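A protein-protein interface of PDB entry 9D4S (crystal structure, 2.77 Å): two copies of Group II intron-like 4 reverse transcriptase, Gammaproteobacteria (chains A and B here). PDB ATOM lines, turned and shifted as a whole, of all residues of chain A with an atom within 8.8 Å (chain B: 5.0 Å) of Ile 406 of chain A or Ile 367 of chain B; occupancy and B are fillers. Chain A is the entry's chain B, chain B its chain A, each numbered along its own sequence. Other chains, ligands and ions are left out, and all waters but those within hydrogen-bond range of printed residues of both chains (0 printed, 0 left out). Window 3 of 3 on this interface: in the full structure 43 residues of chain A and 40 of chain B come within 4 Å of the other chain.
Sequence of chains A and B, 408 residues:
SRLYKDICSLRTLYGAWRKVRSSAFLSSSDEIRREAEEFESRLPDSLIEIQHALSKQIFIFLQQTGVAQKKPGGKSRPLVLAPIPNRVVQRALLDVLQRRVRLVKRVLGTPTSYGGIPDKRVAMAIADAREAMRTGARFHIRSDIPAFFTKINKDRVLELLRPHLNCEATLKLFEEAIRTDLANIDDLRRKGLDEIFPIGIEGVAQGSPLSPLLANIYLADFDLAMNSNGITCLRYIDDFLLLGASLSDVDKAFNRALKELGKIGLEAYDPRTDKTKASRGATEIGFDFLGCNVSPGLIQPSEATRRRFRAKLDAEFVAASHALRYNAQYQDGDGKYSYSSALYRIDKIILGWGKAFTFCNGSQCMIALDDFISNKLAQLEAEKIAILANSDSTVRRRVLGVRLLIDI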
ATOM      1  N   THR A 394      20.355   2.528 -28.268  1.00  0.00           N
ATOM      2  CA  THR A 394      21.121   2.936 -27.058  1.00  0.00           C
ATOM      3  C   THR A 394      22.265   3.885 -27.436  1.00  0.00           C
ATOM      4  O   THR A 394      22.418   4.916 -26.752  1.00  0.00           O
ATOM      5  CB  THR A 394      21.636   1.710 -26.289  1.00  0.00           C
ATOM      6  OG1 THR A 394      22.608   2.159 -25.347  1.00  0.00           O
ATOM      7  CG2 THR A 394      22.246   0.659 -27.190  1.00  0.00           C
ATOM      8  N   ARG A 397      21.091   7.317 -28.304  1.00  0.00           N
ATOM      9  CA  ARG A 397      20.645   7.999 -27.090  1.00  0.00           C
ATOM     10  C   ARG A 397      21.796   8.671 -26.342  1.00  0.00           C
ATOM     11  O   ARG A 397      21.690   9.847 -25.958  1.00  0.00           O
ATOM     12  CB  ARG A 397      19.928   7.000 -26.176  1.00  0.00           C
ATOM     13  CG  ARG A 397      18.574   6.518 -26.695  1.00  0.00           C
ATOM     14  CD  ARG A 397      17.461   7.496 -26.381  1.00  0.00           C
ATOM     15  NE  ARG A 397      17.135   7.525 -24.957  1.00  0.00           N
ATOM     16  CZ  ARG A 397      16.185   6.799 -24.368  1.00  0.00           C
ATOM     17  NH1 ARG A 397      15.450   5.937 -25.052  1.00  0.00           N
ATOM     18  NH2 ARG A 397      15.962   6.956 -23.064  1.00  0.00           N
ATOM     19  N   ARG A 403      19.275  10.785 -22.130  1.00  0.00           N
ATOM     20  CA  ARG A 403      19.593   9.759 -21.142  1.00  0.00           C
ATOM     21  C   ARG A 403      18.696   8.532 -21.251  1.00  0.00           C
ATOM     22  O   ARG A 403      17.523   8.617 -21.636  1.00  0.00           O
ATOM     23  CB  ARG A 403      19.381  10.369 -19.770  1.00  0.00           C
ATOM     24  CG  ARG A 403      20.032   9.751 -18.652  1.00  0.00           C
ATOM     25  CD  ARG A 403      19.895  10.762 -17.588  1.00  0.00           C
ATOM     26  NE  ARG A 403      20.264  12.033 -18.187  1.00  0.00           N
ATOM     27  CZ  ARG A 403      21.099  12.904 -17.644  1.00  0.00           C
ATOM     28  NH1 ARG A 403      21.689  12.663 -16.483  1.00  0.00           N
ATOM     29  NH2 ARG A 403      21.355  14.041 -18.287  1.00  0.00           N
ATOM     30  N   LEU A 404      19.233   7.392 -20.818  1.00  0.00           N
ATOM     31  CA  LEU A 404      18.461   6.156 -20.768  1.00  0.00           C
ATOM     32  C   LEU A 404      17.950   5.967 -19.342  1.00  0.00           C
ATOM     33  O   LEU A 404      18.705   6.139 -18.377  1.00  0.00           O
ATOM     34  CB  LEU A 404      19.307   4.956 -21.216  1.00  0.00           C
ATOM     35  CG  LEU A 404      19.354   4.713 -22.737  1.00  0.00           C
ATOM     36  CD1 LEU A 404      20.595   3.939 -23.164  1.00  0.00           C
ATOM     37  CD2 LEU A 404      18.115   4.028 -23.252  1.00  0.00           C
ATOM     38  N   LEU A 405      16.668   5.617 -19.212  1.00  0.00           N
ATOM     39  CA  LEU A 405      16.106   5.396 -17.883  1.00  0.00           C
ATOM     40  C   LEU A 405      16.733   4.185 -17.212  1.00  0.00           C
ATOM     41  O   LEU A 405      16.981   4.205 -15.998  1.00  0.00           O
ATOM     42  CB  LEU A 405      14.594   5.232 -17.986  1.00  0.00           C
ATOM     43  CG  LEU A 405      13.841   6.543 -18.169  1.00  0.00           C
ATOM     44  CD1 LEU A 405      12.497   6.296 -18.819  1.00  0.00           C
ATOM     45  CD2 LEU A 405      13.691   7.256 -16.833  1.00  0.00           C
ATOM     46  N   ILE A 406      17.059   3.156 -17.999  1.00  0.00           N
ATOM     47  CA  ILE A 406      17.622   1.923 -17.474  1.00  0.00           C
ATOM     48  C   ILE A 406      18.931   2.151 -16.719  1.00  0.00           C
ATOM     49  O   ILE A 406      19.347   1.289 -15.941  1.00  0.00           O
ATOM     50  CB  ILE A 406      17.806   0.931 -18.644  1.00  0.00           C
ATOM     51  CG1 ILE A 406      18.616   1.609 -19.720  1.00  0.00           C
ATOM     52  CG2 ILE A 406      16.502   0.537 -19.295  1.00  0.00           C
ATOM     53  CD1 ILE A 406      19.448   0.694 -20.457  1.00  0.00           C
ATOM     54  N   ASP A 407      19.618   3.272 -16.967  1.00  0.00           N
ATOM     55  CA  ASP A 407      20.919   3.545 -16.361  1.00  0.00           C
ATOM     56  C   ASP A 407      20.876   4.575 -15.228  1.00  0.00           C
ATOM     57  O   ASP A 407      21.933   5.083 -14.842  1.00  0.00           O
ATOM     58  CB  ASP A 407      21.902   4.010 -17.435  1.00  0.00           C
ATOM     59  CG  ASP A 407      22.307   2.899 -18.371  1.00  0.00           C
ATOM     60  OD1 ASP A 407      21.430   2.105 -18.737  1.00  0.00           O
ATOM     61  OD2 ASP A 407      23.488   2.842 -18.785  1.00  0.00           O
ATOM     62  N   ILE A 408      19.730   4.849 -14.630  1.00  0.00           N
ATOM     63  CA  ILE A 408      19.740   5.935 -13.652  1.00  0.00           C
ATOM     64  C   ILE A 408      20.008   5.438 -12.239  1.00  0.00           C
ATOM     65  O   ILE A 408      20.886   5.976 -11.553  1.00  0.00           O
ATOM     66  CB  ILE A 408      18.435   6.733 -13.682  1.00  0.00           C
ATOM     67  CG1 ILE A 408      18.426   7.680 -14.874  1.00  0.00           C
ATOM     68  CG2 ILE A 408      18.278   7.547 -12.403  1.00  0.00           C
ATOM     69  CD1 ILE A 408      17.339   8.688 -14.801  1.00  0.00           C
ATOM     70  N   SER B 363      12.580  -3.130 -13.736  1.00  0.00           N
ATOM     71  CA  SER B 363      13.201  -2.644 -14.961  1.00  0.00           C
ATOM     72  C   SER B 363      12.385  -2.859 -16.232  1.00  0.00           C
ATOM     73  O   SER B 363      12.640  -2.171 -17.224  1.00  0.00           O
ATOM     74  CB  SER B 363      14.570  -3.314 -15.130  1.00  0.00           C
ATOM     75  OG  SER B 363      15.279  -3.271 -13.906  1.00  0.00           O
ATOM     76  N   GLN B 364      11.431  -3.792 -16.242  1.00  0.00           N
ATOM     77  CA  GLN B 364      10.712  -4.102 -17.476  1.00  0.00           C
ATOM     78  C   GLN B 364       9.995  -2.881 -18.034  1.00  0.00           C
ATOM     79  O   GLN B 364      10.052  -2.607 -19.239  1.00  0.00           O
ATOM     80  CB  GLN B 364       9.724  -5.251 -17.240  1.00  0.00           C
ATOM     81  CG  GLN B 364       9.299  -6.026 -18.504  1.00  0.00           C
ATOM     82  CD  GLN B 364       8.356  -7.193 -18.182  1.00  0.00           C
ATOM     83  OE1 GLN B 364       8.293  -7.672 -17.038  1.00  0.00           O
ATOM     84  NE2 GLN B 364       7.617  -7.652 -19.185  1.00  0.00           N
ATOM     85  N   CYS B 365       9.304  -2.135 -17.173  1.00  0.00           N
ATOM     86  CA  CYS B 365       8.541  -0.991 -17.647  1.00  0.00           C
ATOM     87  C   CYS B 365       9.420   0.233 -17.872  1.00  0.00           C
ATOM     88  O   CYS B 365       9.160   1.009 -18.798  1.00  0.00           O
ATOM     89  CB  CYS B 365       7.402  -0.702 -16.660  1.00  0.00           C
ATOM     90  SG  CYS B 365       5.799  -1.590 -17.089  1.00  0.00           S
ATOM     91  N   MET B 366      10.487   0.390 -17.089  1.00  0.00           N
ATOM     92  CA  MET B 366      11.554   1.321 -17.435  1.00  0.00           C
ATOM     93  C   MET B 366      12.122   1.041 -18.830  1.00  0.00           C
ATOM     94  O   MET B 366      12.419   1.975 -19.586  1.00  0.00           O
ATOM     95  CB  MET B 366      12.652   1.265 -16.368  1.00  0.00           C
ATOM     96  CG  MET B 366      12.973   2.627 -15.814  1.00  0.00           C
ATOM     97  SD  MET B 366      11.569   3.311 -14.891  1.00  0.00           S
ATOM     98  CE  MET B 366      11.989   2.961 -13.182  1.00  0.00           C
ATOM     99  N   ILE B 367      12.255  -0.235 -19.203  1.00  0.00           N
ATOM    100  CA  ILE B 367      12.815  -0.548 -20.519  1.00  0.00           C
ATOM    101  C   ILE B 367      11.813  -0.208 -21.615  1.00  0.00           C
ATOM    102  O   ILE B 367      12.181   0.332 -22.667  1.00  0.00           O
ATOM    103  CB  ILE B 367      13.246  -2.030 -20.583  1.00  0.00           C
ATOM    104  CG1 ILE B 367      14.602  -2.236 -19.922  1.00  0.00           C
ATOM    105  CG2 ILE B 367      13.303  -2.538 -22.011  1.00  0.00           C
ATOM    106  CD1 ILE B 367      14.730  -3.559 -19.231  1.00  0.00           C
ATOM    107  N   ALA B 368      10.535  -0.486 -21.381  1.00  0.00           N
ATOM    108  CA  ALA B 368       9.512  -0.139 -22.356  1.00  0.00           C
ATOM    109  C   ALA B 368       9.394   1.371 -22.531  1.00  0.00           C
ATOM    110  O   ALA B 368       9.229   1.861 -23.653  1.00  0.00           O
ATOM    111  CB  ALA B 368       8.169  -0.731 -21.932  1.00  0.00           C
ATOM    112  N   LEU B 369       9.462   2.126 -21.431  1.00  0.00           N
ATOM    113  CA  LEU B 369       9.503   3.581 -21.543  1.00  0.00           C
ATOM    114  C   LEU B 369      10.762   4.043 -22.277  1.00  0.00           C
ATOM    115  O   LEU B 369      10.702   4.960 -23.097  1.00  0.00           O
ATOM    116  CB  LEU B 369       9.384   4.230 -20.161  1.00  0.00           C
ATOM    117  CG  LEU B 369       7.903   4.459 -19.829  1.00  0.00           C
ATOM    118  CD1 LEU B 369       7.679   4.888 -18.381  1.00  0.00           C
ATOM    119  CD2 LEU B 369       7.265   5.461 -20.806  1.00  0.00           C
ATOM    120  N   ASP B 370      11.908   3.408 -22.009  1.00  0.00           N
ATOM    121  CA  ASP B 370      13.102   3.744 -22.772  1.00  0.00           C
ATOM    122  C   ASP B 370      12.909   3.450 -24.255  1.00  0.00           C
ATOM    123  O   ASP B 370      13.320   4.242 -25.107  1.00  0.00           O
ATOM    124  CB  ASP B 370      14.312   2.983 -22.241  1.00  0.00           C
ATOM    125  CG  ASP B 370      15.172   3.832 -21.326  1.00  0.00           C
ATOM    126  OD1 ASP B 370      15.270   5.053 -21.573  1.00  0.00           O
ATOM    127  OD2 ASP B 370      15.761   3.282 -20.365  1.00  0.00           O
ATOM    128  N   ASP B 371      12.209   2.368 -24.585  1.00  0.00           N
ATOM    129  CA  ASP B 371      12.006   2.057 -25.995  1.00  0.00           C
ATOM    130  C   ASP B 371      11.172   3.137 -26.668  1.00  0.00           C
ATOM    131  O   ASP B 371      11.539   3.640 -27.732  1.00  0.00           O
ATOM    132  CB  ASP B 371      11.337   0.690 -26.155  1.00  0.00           C
ATOM    133  CG  ASP B 371      12.270  -0.464 -25.813  1.00  0.00           C
ATOM    134  OD1 ASP B 371      13.419  -0.209 -25.380  1.00  0.00           O
ATOM    135  OD2 ASP B 371      11.844  -1.633 -25.979  1.00  0.00           O
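OD2 of Asp 370 of chain B is in hydrogen-bond range of N of Leu 405 of chain A (2.8 Å).
The side-chain carboxylate (OD1) of Asp 370 of chain B is in salt-bridge range of the guanidinium group (NH2) of Arg 397 of chain A, 2.5 Å away.
OD2 of Asp 370 of chain B is in hydrogen-bond range of N of Ile 406 of chain A (2.7 Å).
NH2 of Arg 397 of chain A sits at hydrogen-bond distance from O of Arg 403 of chain A (2.7 Å).
Asp 370 of chain B touches Leu 404 of chain A.
Leu 405 of chain A touches Met 366 of chain B.
Leu 369 of chain B touches Leu 405 of chain A.
Ile 367 of chain B touches Ile 406 of chain A (CG1 to CG2, 3.4 Å).
Of the printed residues of chain B, Arg 397 of chain A touches Asp 370.
Printed residues of chain B within 4 Å of Leu 404 of chain A: Asp 370 (3.5 Å).
Of the printed residues of chain B, Leu 405 of chain A touches Met 366 (3.8 Å), Leu 369 (3.97 Å) and Asp 370 (2.8 Å).
Of chain B, only Ile 367 (3.4 Å) and Asp 370 (2.7 Å) come within 4 Å of Ile 406 of chain A.
Gln 364 of chain B touches none of the printed residues of chain A.
Printed residues of chain A within 4 Å of Met 366 of chain B: Leu 405.
Ile 367 of chain B touches just one residue of chain A: Ile 406 (3.4 Å).
No residue of chain A comes within 4 Å of Ala 368 of chain B.
Printed residues of chain A within 4 Å of Leu 369 of chain B: Leu 405 (3.97 Å).
Asp 370 of chain B touches four residues of chain A.
The nearest residue of chain B that does not touch Ile 406 of chain A is Met 366 of chain B (4.3 Å).
Of the 8 printed residues of chain A, 4 touch a printed residue of chain B.
Hydrophobic or aromatic side chains of chain A that line the printed part of chain B: Leu 404, Leu 405 and Ile 406.
Hydrophobic or aromatic side chains of chain B within 4 Å of the printed part of chain A: Met 366, Ile 367 and Leu 369.
Among the printed residues, Asp or Glu carboxylates within 4 Å of a Lys or Arg side-chain nitrogen of the other chain: Arg 397 of chain A with Asp 370 of chain B.
No position is printed for both chains.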
